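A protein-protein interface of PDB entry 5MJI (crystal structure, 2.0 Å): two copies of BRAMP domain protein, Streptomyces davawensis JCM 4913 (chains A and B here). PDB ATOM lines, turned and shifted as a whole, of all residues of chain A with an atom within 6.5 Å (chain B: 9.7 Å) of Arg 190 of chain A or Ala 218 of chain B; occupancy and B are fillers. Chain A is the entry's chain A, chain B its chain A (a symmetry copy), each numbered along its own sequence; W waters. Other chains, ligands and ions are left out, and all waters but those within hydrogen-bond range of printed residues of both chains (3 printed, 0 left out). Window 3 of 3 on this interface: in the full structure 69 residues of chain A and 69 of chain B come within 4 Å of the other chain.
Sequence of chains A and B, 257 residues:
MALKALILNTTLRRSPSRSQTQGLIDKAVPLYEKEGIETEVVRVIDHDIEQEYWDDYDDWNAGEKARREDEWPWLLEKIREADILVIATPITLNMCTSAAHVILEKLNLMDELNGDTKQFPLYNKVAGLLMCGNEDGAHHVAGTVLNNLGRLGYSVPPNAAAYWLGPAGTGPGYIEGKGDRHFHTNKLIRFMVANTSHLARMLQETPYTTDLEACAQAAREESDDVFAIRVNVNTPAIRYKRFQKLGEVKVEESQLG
The side-chain amide nitrogen of Asn 186 of chain A lies within hydrogen-bond range of the side-chain hydroxyl of Ser 223 of chain B. The guanidinium group (NE) of Arg 190 of chain A lies within salt-bridge range of the side-chain carboxylate (OE2) of Glu 222 of chain B. The side-chain amide nitrogen (ND2) of Asn 195 of chain A is in hydrogen-bond range of the side-chain hydroxyl (OH) of Tyr 123 of chain B (2.8 Å). The side-chain amide oxygen of Asn 195 of chain A lies within hydrogen-bond range of the side-chain hydroxyl of Thr 210 of chain B (2.6 Å).
The backbone carbonyl oxygen of Phe 191 of chain A lies close to the side-chain amide nitrogen of Asn 195 of chain A (3.5 Å). O of Asp 211 of chain B is in hydrogen-bond range of SG of Cys 215 of chain B (3.6 Å). The backbone carbonyl oxygen of Ala 219 of chain B is in hydrogen-bond range of the side-chain hydroxyl of Ser 223 of chain B (2.5 Å). NH1 of Arg 220 of chain B is in salt-bridge range of OE2 of Glu 221 of chain B (3.2 Å).
CD1 of Phe 183 of chain A touches C of Ala 219 of chain B (3.8 Å). Phe 183 of chain A touches Arg 220 of chain B (CE1 to N, 3.6 Å). Phe 183 of chain A touches Ser 223 of chain B. Ala 219 of chain B touches Asn 186 of chain A. N of Lys 187 of chain A touches CB of Ala 219 of chain B, 3.5 Å away. Arg 190 of chain A touches Cys 215 of chain B. CZ of Arg 190 of chain A touches CB of Ala 218 of chain B (3.4 Å). Leu 212 of chain B touches Phe 191 of chain A. Phe 191 of chain A touches Cys 215 of chain B (CE1 to CB, 3.5 Å). Ala 194 of chain A touches Thr 210 of chain B.
Of the printed residues of chain A, Ala 218 of chain B touches Arg 190 (3.4 Å). Ile 189 of chain A touches none of the printed residues of chain B. No residue of chain B comes within 4 Å of Val 193 of chain A. Of the printed residues of chain A, Glu 222 of chain B touches Asn 186 (3.5 Å) and Arg 190 (3.0 Å). Of the printed residues of chain B, Asn 186 of chain A touches Ala 219 (3.9 Å), Glu 222 (3.5 Å) and Ser 223 (3.0 Å). Printed residues of chain A within 4 Å of Cys 215 of chain B: Arg 190 (3.3 Å) and Phe 191 (3.5 Å). Printed residues of chain A within 4 Å of Thr 210 of chain B: Ala 194 (3.6 Å) and Asn 195 (2.6 Å). Of the printed residues of chain A, Tyr 123 of chain B touches Asn 195. The nearest residue of chain B that does not touch Arg 190 of chain A is Ala 216 of chain B (5.4 Å).
Hydrophobic or aromatic side chains of chain A that line the printed part of chain B: Phe 183, Phe 191 and Ala 194. Of the 16 printed residues of chain B, 10 touch a printed residue of chain A. Hydrophobic or aromatic side chains of chain B within 4 Å of the printed part of chain A: Tyr 123, Leu 212, Ala 218 and Ala 219. Along chain B the printed residues that touch a printed residue of chain A span positions 123 to 223.
No position is printed for both chains. Of the 17 pairs that touch across the chains among the printed residues, none has its exchanged pair printed and touching as well.
Water W2 lies within hydrogen-bond range of N of Phe 183 of chain A (2.7 Å) and O of Asp 224 of chain B (2.8 Å). Water W3 bridges OE1 of Glu 222 of chain B (2.9 Å) and NH2 of Arg 190 of chain A (3.4 Å). Water W1 lies within hydrogen-bond range of the backbone carbonyl oxygen (O) of Asn 186 of chain A (2.9 Å) and the side-chain carboxylate (OE2) of Glu 222 of chain B (3.4 Å).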
ATOM      1  N   LEU A  31     -13.299  17.865  10.363  1.00  0.00           N
ATOM      2  CA  LEU A  31     -13.929  16.943   9.416  1.00  0.00           C
ATOM      3  C   LEU A  31     -15.328  17.409   9.042  1.00  0.00           C
ATOM      4  O   LEU A  31     -15.736  17.307   7.875  1.00  0.00           O
ATOM      5  CB  LEU A  31     -13.981  15.532   9.999  1.00  0.00           C
ATOM      6  CG  LEU A  31     -12.636  14.876  10.293  1.00  0.00           C
ATOM      7  CD1 LEU A  31     -12.780  13.664  11.213  1.00  0.00           C
ATOM      8  CD2 LEU A  31     -11.968  14.490   8.976  1.00  0.00           C
ATOM      9  N   LYS A  34     -15.007  20.398   6.557  1.00  0.00           N
ATOM     10  CA  LYS A  34     -14.744  19.965   5.187  1.00  0.00           C
ATOM     11  C   LYS A  34     -15.976  19.351   4.533  1.00  0.00           C
ATOM     12  O   LYS A  34     -16.091  19.370   3.305  1.00  0.00           O
ATOM     13  CB  LYS A  34     -13.580  18.980   5.135  1.00  0.00           C
ATOM     14  CG  LYS A  34     -12.276  19.558   5.647  1.00  0.00           C
ATOM     15  CD  LYS A  34     -11.276  18.445   5.852  1.00  0.00           C
ATOM     16  CE  LYS A  34     -10.430  18.643   7.102  1.00  0.00           C
ATOM     17  NZ  LYS A  34      -9.837  17.330   7.468  1.00  0.00           N
ATOM     18  N   GLU A  35     -16.897  18.796   5.322  1.00  0.00           N
ATOM     19  CA  GLU A  35     -18.201  18.409   4.798  1.00  0.00           C
ATOM     20  C   GLU A  35     -19.066  19.609   4.459  1.00  0.00           C
ATOM     21  O   GLU A  35     -20.203  19.420   4.010  1.00  0.00           O
ATOM     22  CB  GLU A  35     -18.952  17.530   5.809  1.00  0.00           C
ATOM     23  CG  GLU A  35     -18.380  16.156   5.997  1.00  0.00           C
ATOM     24  CD  GLU A  35     -18.831  15.187   4.930  1.00  0.00           C
ATOM     25  OE1 GLU A  35     -19.614  15.596   4.045  1.00  0.00           O
ATOM     26  OE2 GLU A  35     -18.416  14.011   4.977  1.00  0.00           O
ATOM     27  N   ALA A 162     -18.325   7.110  18.145  1.00  0.00           N
ATOM     28  CA  ALA A 162     -16.875   7.014  18.099  1.00  0.00           C
ATOM     29  C   ALA A 162     -16.333   7.275  19.496  1.00  0.00           C
ATOM     30  O   ALA A 162     -16.900   8.069  20.244  1.00  0.00           O
ATOM     31  CB  ALA A 162     -16.286   8.017  17.106  1.00  0.00           C
ATOM     32  N   PHE A 183      -5.434   4.582  16.183  1.00  0.00           N
ATOM     33  CA  PHE A 183      -5.981   4.342  14.853  1.00  0.00           C
ATOM     34  C   PHE A 183      -7.481   4.075  14.903  1.00  0.00           C
ATOM     35  O   PHE A 183      -8.255   4.622  14.106  1.00  0.00           O
ATOM     36  CB  PHE A 183      -5.254   3.169  14.208  1.00  0.00           C
ATOM     37  CG  PHE A 183      -5.916   2.662  12.951  1.00  0.00           C
ATOM     38  CD1 PHE A 183      -5.912   3.433  11.794  1.00  0.00           C
ATOM     39  CD2 PHE A 183      -6.516   1.414  12.925  1.00  0.00           C
ATOM     40  CE1 PHE A 183      -6.506   2.976  10.626  1.00  0.00           C
ATOM     41  CE2 PHE A 183      -7.124   0.947  11.758  1.00  0.00           C
ATOM     42  CZ  PHE A 183      -7.116   1.738  10.604  1.00  0.00           C
ATOM     43  N   THR A 185      -9.852   4.798  17.132  1.00  0.00           N
ATOM     44  CA  THR A 185     -10.661   5.976  17.437  1.00  0.00           C
ATOM     45  C   THR A 185     -10.704   6.923  16.252  1.00  0.00           C
ATOM     46  O   THR A 185     -11.768   7.427  15.885  1.00  0.00           O
ATOM     47  CB  THR A 185     -10.100   6.713  18.653  1.00  0.00           C
ATOM     48  OG1 THR A 185     -10.096   5.838  19.790  1.00  0.00           O
ATOM     49  CG2 THR A 185     -10.938   7.975  18.951  1.00  0.00           C
ATOM     50  N   ASN A 186      -9.546   7.163  15.631  1.00  0.00           N
ATOM     51  CA  ASN A 186      -9.502   8.087  14.510  1.00  0.00           C
ATOM     52  C   ASN A 186     -10.351   7.590  13.350  1.00  0.00           C
ATOM     53  O   ASN A 186     -11.024   8.382  12.685  1.00  0.00           O
ATOM     54  CB  ASN A 186      -8.052   8.319  14.087  1.00  0.00           C
ATOM     55  CG  ASN A 186      -7.365   9.315  14.988  1.00  0.00           C
ATOM     56  OD1 ASN A 186      -8.004  10.242  15.480  1.00  0.00           O
ATOM     57  ND2 ASN A 186      -6.085   9.128  15.230  1.00  0.00           N
ATOM     58  N   LYS A 187     -10.372   6.283  13.102  1.00  0.00           N
ATOM     59  CA  LYS A 187     -11.196   5.868  11.979  1.00  0.00           C
ATOM     60  C   LYS A 187     -12.670   5.941  12.341  1.00  0.00           C
ATOM     61  O   LYS A 187     -13.491   6.327  11.498  1.00  0.00           O
ATOM     62  CB  LYS A 187     -10.768   4.484  11.479  1.00  0.00           C
ATOM     63  CG  LYS A 187     -11.405   3.276  12.111  1.00  0.00           C
ATOM     64  CD  LYS A 187     -10.850   2.016  11.449  1.00  0.00           C
ATOM     65  CE  LYS A 187     -11.317   0.763  12.127  1.00  0.00           C
ATOM     66  NZ  LYS A 187     -10.465  -0.415  11.757  1.00  0.00           N
ATOM     67  N   LEU A 188     -13.020   5.655  13.603  1.00  0.00           N
ATOM     68  CA  LEU A 188     -14.432   5.711  13.982  1.00  0.00           C
ATOM     69  C   LEU A 188     -14.966   7.130  13.877  1.00  0.00           C
ATOM     70  O   LEU A 188     -16.118   7.337  13.480  1.00  0.00           O
ATOM     71  CB  LEU A 188     -14.645   5.188  15.398  1.00  0.00           C
ATOM     72  CG  LEU A 188     -14.410   3.702  15.679  1.00  0.00           C
ATOM     73  CD1 LEU A 188     -14.860   3.417  17.095  1.00  0.00           C
ATOM     74  CD2 LEU A 188     -15.161   2.852  14.678  1.00  0.00           C
ATOM     75  N   ILE A 189     -14.151   8.117  14.267  1.00  0.00           N
ATOM     76  CA  ILE A 189     -14.574   9.510  14.163  1.00  0.00           C
ATOM     77  C   ILE A 189     -14.847   9.866  12.711  1.00  0.00           C
ATOM     78  O   ILE A 189     -15.857  10.504  12.393  1.00  0.00           O
ATOM     79  CB  ILE A 189     -13.516  10.439  14.787  1.00  0.00           C
ATOM     80  CG1 ILE A 189     -13.456  10.212  16.304  1.00  0.00           C
ATOM     81  CG2 ILE A 189     -13.781  11.926  14.407  1.00  0.00           C
ATOM     82  CD1 ILE A 189     -12.275  10.884  16.980  1.00  0.00           C
ATOM     83  N   ARG A 190     -13.974   9.427  11.804  1.00  0.00           N
ATOM     84  CA  ARG A 190     -14.198   9.692  10.389  1.00  0.00           C
ATOM     85  C   ARG A 190     -15.468   9.016   9.897  1.00  0.00           C
ATOM     86  O   ARG A 190     -16.262   9.644   9.189  1.00  0.00           O
ATOM     87  CB  ARG A 190     -12.984   9.253   9.570  1.00  0.00           C
ATOM     88  CG  ARG A 190     -11.744  10.059   9.918  1.00  0.00           C
ATOM     89  CD  ARG A 190     -10.556   9.689   9.051  1.00  0.00           C
ATOM     90  NE  ARG A 190      -9.443  10.610   9.262  1.00  0.00           N
ATOM     91  CZ  ARG A 190      -9.214  11.698   8.526  1.00  0.00           C
ATOM     92  NH1 ARG A 190     -10.015  12.002   7.517  1.00  0.00           N
ATOM     93  NH2 ARG A 190      -8.172  12.475   8.797  1.00  0.00           N
ATOM     94  N   PHE A 191     -15.710   7.760  10.304  1.00  0.00           N
ATOM     95  CA  PHE A 191     -16.980   7.109   9.966  1.00  0.00           C
ATOM     96  C   PHE A 191     -18.168   7.947  10.434  1.00  0.00           C
ATOM     97  O   PHE A 191     -19.104   8.205   9.668  1.00  0.00           O
ATOM     98  CB  PHE A 191     -17.093   5.716  10.605  1.00  0.00           C
ATOM     99  CG  PHE A 191     -16.095   4.695  10.117  1.00  0.00           C
ATOM    100  CD1 PHE A 191     -15.192   4.979   9.107  1.00  0.00           C
ATOM    101  CD2 PHE A 191     -16.069   3.430  10.698  1.00  0.00           C
ATOM    102  CE1 PHE A 191     -14.285   4.014   8.676  1.00  0.00           C
ATOM    103  CE2 PHE A 191     -15.166   2.470  10.280  1.00  0.00           C
ATOM    104  CZ  PHE A 191     -14.271   2.763   9.256  1.00  0.00           C
ATOM    105  N   MET A 192     -18.145   8.357  11.709  1.00  0.00           N
ATOM    106  CA  MET A 192     -19.264   9.101  12.289  1.00  0.00           C
ATOM    107  C   MET A 192     -19.532  10.390  11.522  1.00  0.00           C
ATOM    108  O   MET A 192     -20.686  10.700  11.186  1.00  0.00           O
ATOM    109  CB  MET A 192     -18.985   9.418  13.769  1.00  0.00           C
ATOM    110  CG  MET A 192     -20.070  10.283  14.454  1.00  0.00           C
ATOM    111  SD  MET A 192     -19.593  10.955  16.079  1.00  0.00           S
ATOM    112  CE  MET A 192     -18.719  12.433  15.555  1.00  0.00           C
ATOM    113  N   VAL A 193     -18.483  11.168  11.247  1.00  0.00           N
ATOM    114  CA  VAL A 193     -18.691  12.456  10.594  1.00  0.00           C
ATOM    115  C   VAL A 193     -19.297  12.249   9.213  1.00  0.00           C
ATOM    116  O   VAL A 193     -20.282  12.897   8.840  1.00  0.00           O
ATOM    117  CB  VAL A 193     -17.377  13.247  10.521  1.00  0.00           C
ATOM    118  CG1 VAL A 193     -17.601  14.527   9.724  1.00  0.00           C
ATOM    119  CG2 VAL A 193     -16.863  13.563  11.930  1.00  0.00           C
ATOM    120  N   ALA A 194     -18.736  11.317   8.447  1.00  0.00           N
ATOM    121  CA  ALA A 194     -19.229  11.091   7.092  1.00  0.00           C
ATOM    122  C   ALA A 194     -20.674  10.612   7.107  1.00  0.00           C
ATOM    123  O   ALA A 194     -21.487  11.059   6.293  1.00  0.00           O
ATOM    124  CB  ALA A 194     -18.339  10.081   6.375  1.00  0.00           C
ATOM    125  N   ASN A 195     -21.018   9.711   8.035  1.00  0.00           N
ATOM    126  CA  ASN A 195     -22.366   9.145   8.018  1.00  0.00           C
ATOM    127  C   ASN A 195     -23.399  10.115   8.583  1.00  0.00           C
ATOM    128  O   ASN A 195     -24.506  10.209   8.049  1.00  0.00           O
ATOM    129  CB  ASN A 195     -22.390   7.813   8.774  1.00  0.00           C
ATOM    130  CG  ASN A 195     -21.608   6.721   8.048  1.00  0.00           C
ATOM    131  OD1 ASN A 195     -21.298   6.846   6.859  1.00  0.00           O
ATOM    132  ND2 ASN A 195     -21.293   5.646   8.757  1.00  0.00           N
ATOM    133  N   TYR B 123     -24.745  -2.114   5.143  1.00  0.00           N
ATOM    134  CA  TYR B 123     -24.947  -0.683   4.976  1.00  0.00           C
ATOM    135  C   TYR B 123     -26.202  -0.396   4.170  1.00  0.00           C
ATOM    136  O   TYR B 123     -26.624  -1.193   3.321  1.00  0.00           O
ATOM    137  CB  TYR B 123     -23.737  -0.046   4.289  1.00  0.00           C
ATOM    138  CG  TYR B 123     -22.925   0.792   5.237  1.00  0.00           C
ATOM    139  CD1 TYR B 123     -22.325   0.209   6.345  1.00  0.00           C
ATOM    140  CD2 TYR B 123     -22.754   2.168   5.030  1.00  0.00           C
ATOM    141  CE1 TYR B 123     -21.571   0.954   7.230  1.00  0.00           C
ATOM    142  CE2 TYR B 123     -21.999   2.933   5.925  1.00  0.00           C
ATOM    143  CZ  TYR B 123     -21.420   2.316   7.026  1.00  0.00           C
ATOM    144  OH  TYR B 123     -20.657   3.027   7.925  1.00  0.00           O
ATOM    145  N   THR B 210     -20.248   7.048   1.809  1.00  0.00           N
ATOM    146  CA  THR B 210     -19.044   6.903   2.616  1.00  0.00           C
ATOM    147  C   THR B 210     -18.157   5.769   2.113  1.00  0.00           C
ATOM    148  O   THR B 210     -18.630   4.662   1.856  1.00  0.00           O
ATOM    149  CB  THR B 210     -19.440   6.629   4.065  1.00  0.00           C
ATOM    150  OG1 THR B 210     -20.446   7.566   4.468  1.00  0.00           O
ATOM    151  CG2 THR B 210     -18.217   6.735   4.970  1.00  0.00           C
ATOM    152  N   ASP B 211     -16.868   6.052   1.991  1.00  0.00           N
ATOM    153  CA  ASP B 211     -15.855   5.067   1.608  1.00  0.00           C
ATOM    154  C   ASP B 211     -15.058   4.740   2.869  1.00  0.00           C
ATOM    155  O   ASP B 211     -14.161   5.496   3.257  1.00  0.00           O
ATOM    156  CB  ASP B 211     -14.966   5.619   0.488  1.00  0.00           C
ATOM    157  CG  ASP B 211     -13.909   4.619   0.006  1.00  0.00           C
ATOM    158  OD1 ASP B 211     -13.456   3.749   0.792  1.00  0.00           O
ATOM    159  OD2 ASP B 211     -13.510   4.724  -1.171  1.00  0.00           O
ATOM    160  N   LEU B 212     -15.384   3.605   3.503  1.00  0.00           N
ATOM    161  CA  LEU B 212     -14.773   3.275   4.791  1.00  0.00           C
ATOM    162  C   LEU B 212     -13.288   2.983   4.649  1.00  0.00           C
ATOM    163  O   LEU B 212     -12.521   3.192   5.596  1.00  0.00           O
ATOM    164  CB  LEU B 212     -15.469   2.070   5.426  1.00  0.00           C
ATOM    165  CG  LEU B 212     -16.970   2.156   5.695  1.00  0.00           C
ATOM    166  CD1 LEU B 212     -17.465   0.835   6.262  1.00  0.00           C
ATOM    167  CD2 LEU B 212     -17.276   3.296   6.660  1.00  0.00           C
ATOM    168  N   GLU B 213     -12.871   2.459   3.497  1.00  0.00           N
ATOM    169  CA  GLU B 213     -11.445   2.258   3.255  1.00  0.00           C
ATOM    170  C   GLU B 213     -10.724   3.585   3.191  1.00  0.00           C
ATOM    171  O   GLU B 213      -9.650   3.750   3.783  1.00  0.00           O
ATOM    172  CB  GLU B 213     -11.229   1.492   1.950  1.00  0.00           C
ATOM    173  CG  GLU B 213     -11.045   0.016   2.122  1.00  0.00           C
ATOM    174  CD  GLU B 213     -10.693  -0.664   0.810  1.00  0.00           C
ATOM    175  OE1 GLU B 213     -10.392   0.054  -0.177  1.00  0.00           O
ATOM    176  OE2 GLU B 213     -10.722  -1.914   0.775  1.00  0.00           O
ATOM    177  N   ALA B 214     -11.305   4.547   2.466  1.00  0.00           N
ATOM    178  CA  ALA B 214     -10.742   5.890   2.435  1.00  0.00           C
ATOM    179  C   ALA B 214     -10.667   6.484   3.839  1.00  0.00           C
ATOM    180  O   ALA B 214      -9.644   7.073   4.216  1.00  0.00           O
ATOM    181  CB  ALA B 214     -11.563   6.781   1.504  1.00  0.00           C
ATOM    182  N   CYS B 215     -11.733   6.333   4.637  1.00  0.00           N
ATOM    183  CA  CYS B 215     -11.668   6.821   6.016  1.00  0.00           C
ATOM    184  C   CYS B 215     -10.537   6.149   6.784  1.00  0.00           C
ATOM    185  O   CYS B 215      -9.798   6.813   7.522  1.00  0.00           O
ATOM    186  CB  CYS B 215     -13.002   6.597   6.731  1.00  0.00           C
ATOM    187  SG  CYS B 215     -14.358   7.637   6.113  1.00  0.00           S
ATOM    188  N   ALA B 216     -10.363   4.837   6.599  1.00  0.00           N
ATOM    189  CA  ALA B 216      -9.338   4.123   7.355  1.00  0.00           C
ATOM    190  C   ALA B 216      -7.932   4.507   6.901  1.00  0.00           C
ATOM    191  O   ALA B 216      -7.006   4.570   7.719  1.00  0.00           O
ATOM    192  CB  ALA B 216      -9.545   2.615   7.229  1.00  0.00           C
ATOM    193  N   GLN B 217      -7.742   4.752   5.601  1.00  0.00           N
ATOM    194  CA  GLN B 217      -6.413   5.143   5.129  1.00  0.00           C
ATOM    195  C   GLN B 217      -6.014   6.498   5.699  1.00  0.00           C
ATOM    196  O   GLN B 217      -4.868   6.689   6.122  1.00  0.00           O
ATOM    197  CB  GLN B 217      -6.380   5.163   3.600  1.00  0.00           C
ATOM    198  CG  GLN B 217      -6.501   3.779   2.972  1.00  0.00           C
ATOM    199  CD  GLN B 217      -6.762   3.840   1.478  1.00  0.00           C
ATOM    200  OE1 GLN B 217      -6.754   4.918   0.877  1.00  0.00           O
ATOM    201  NE2 GLN B 217      -6.965   2.681   0.866  1.00  0.00           N
ATOM    202  N   ALA B 218      -6.952   7.450   5.736  1.00  0.00           N
ATOM    203  CA  ALA B 218      -6.680   8.732   6.378  1.00  0.00           C
ATOM    204  C   ALA B 218      -6.388   8.544   7.863  1.00  0.00           C
ATOM    205  O   ALA B 218      -5.480   9.182   8.413  1.00  0.00           O
ATOM    206  CB  ALA B 218      -7.858   9.687   6.173  1.00  0.00           C
ATOM    207  N   ALA B 219      -7.123   7.646   8.526  1.00  0.00           N
ATOM    208  CA  ALA B 219      -6.853   7.402   9.938  1.00  0.00           C
ATOM    209  C   ALA B 219      -5.475   6.785  10.131  1.00  0.00           C
ATOM    210  O   ALA B 219      -4.782   7.100  11.104  1.00  0.00           O
ATOM    211  CB  ALA B 219      -7.939   6.511  10.542  1.00  0.00           C
ATOM    212  N   ARG B 220      -5.052   5.914   9.212  1.00  0.00           N
ATOM    213  CA  ARG B 220      -3.719   5.325   9.329  1.00  0.00           C
ATOM    214  C   ARG B 220      -2.633   6.390   9.246  1.00  0.00           C
ATOM    215  O   ARG B 220      -1.649   6.348   9.996  1.00  0.00           O
ATOM    216  CB  ARG B 220      -3.510   4.271   8.248  1.00  0.00           C
ATOM    217  CG  ARG B 220      -2.097   3.691   8.207  1.00  0.00           C
ATOM    218  CD  ARG B 220      -1.630   3.564   6.767  1.00  0.00           C
ATOM    219  NE  ARG B 220      -2.339   2.498   6.092  1.00  0.00           N
ATOM    220  CZ  ARG B 220      -2.726   2.532   4.819  1.00  0.00           C
ATOM    221  NH1 ARG B 220      -2.496   3.601   4.061  1.00  0.00           N
ATOM    222  NH2 ARG B 220      -3.375   1.496   4.318  1.00  0.00           N
ATOM    223  N   GLU B 221      -2.796   7.362   8.348  1.00  0.00           N
ATOM    224  CA  GLU B 221      -1.762   8.383   8.180  1.00  0.00           C
ATOM    225  C   GLU B 221      -1.578   9.241   9.423  1.00  0.00           C
ATOM    226  O   GLU B 221      -0.502   9.809   9.609  1.00  0.00           O
ATOM    227  CB  GLU B 221      -2.087   9.285   6.987  1.00  0.00           C
ATOM    228  CG  GLU B 221      -2.167   8.551   5.661  1.00  0.00           C
ATOM    229  CD  GLU B 221      -1.023   7.564   5.474  1.00  0.00           C
ATOM    230  OE1 GLU B 221       0.149   7.957   5.693  1.00  0.00           O
ATOM    231  OE2 GLU B 221      -1.302   6.390   5.124  1.00  0.00           O
ATOM    232  N   GLU B 222      -2.592   9.349  10.281  1.00  0.00           N
ATOM    233  CA  GLU B 222      -2.528  10.225  11.446  1.00  0.00           C
ATOM    234  C   GLU B 222      -2.411   9.444  12.754  1.00  0.00           C
ATOM    235  O   GLU B 222      -2.585  10.021  13.834  1.00  0.00           O
ATOM    236  CB  GLU B 222      -3.752  11.145  11.478  1.00  0.00           C
ATOM    237  CG  GLU B 222      -5.038  10.381  11.788  1.00  0.00           C
ATOM    238  CD  GLU B 222      -6.320  11.156  11.506  1.00  0.00           C
ATOM    239  OE1 GLU B 222      -6.277  12.393  11.355  1.00  0.00           O
ATOM    240  OE2 GLU B 222      -7.385  10.505  11.439  1.00  0.00           O
ATOM    241  N   SER B 223      -2.078   8.155  12.687  1.00  0.00           N
ATOM    242  CA  SER B 223      -2.096   7.287  13.857  1.00  0.00           C
ATOM    243  C   SER B 223      -0.825   6.443  13.938  1.00  0.00           C
ATOM    244  O   SER B 223      -0.071   6.318  12.971  1.00  0.00           O
ATOM    245  CB  SER B 223      -3.340   6.368  13.828  1.00  0.00           C
ATOM    246  OG  SER B 223      -4.542   7.112  13.592  1.00  0.00           O
ATOM    247  N   ASP B 224      -0.598   5.866  15.119  1.00  0.00           N
ATOM    248  CA  ASP B 224       0.426   4.860  15.372  1.00  0.00           C
ATOM    249  C   ASP B 224      -0.124   3.454  15.122  1.00  0.00           C
ATOM    250  O   ASP B 224      -1.338   3.234  15.092  1.00  0.00           O
ATOM    251  CB  ASP B 224       0.926   4.936  16.824  1.00  0.00           C
ATOM    252  CG  ASP B 224       1.419   6.308  17.216  1.00  0.00           C
ATOM    253  OD1 ASP B 224       1.948   7.032  16.343  1.00  0.00           O
ATOM    254  OD2 ASP B 224       1.272   6.661  18.417  1.00  0.00           O
HETATM  255  O   HOH W   1     -10.153  11.095  13.388  1.00  0.00           O
HETATM  256  O   HOH W   2      -3.401   2.902  16.945  1.00  0.00           O
HETATM  257  O   HOH W   3      -8.957  13.217  12.037  1.00  0.00           O
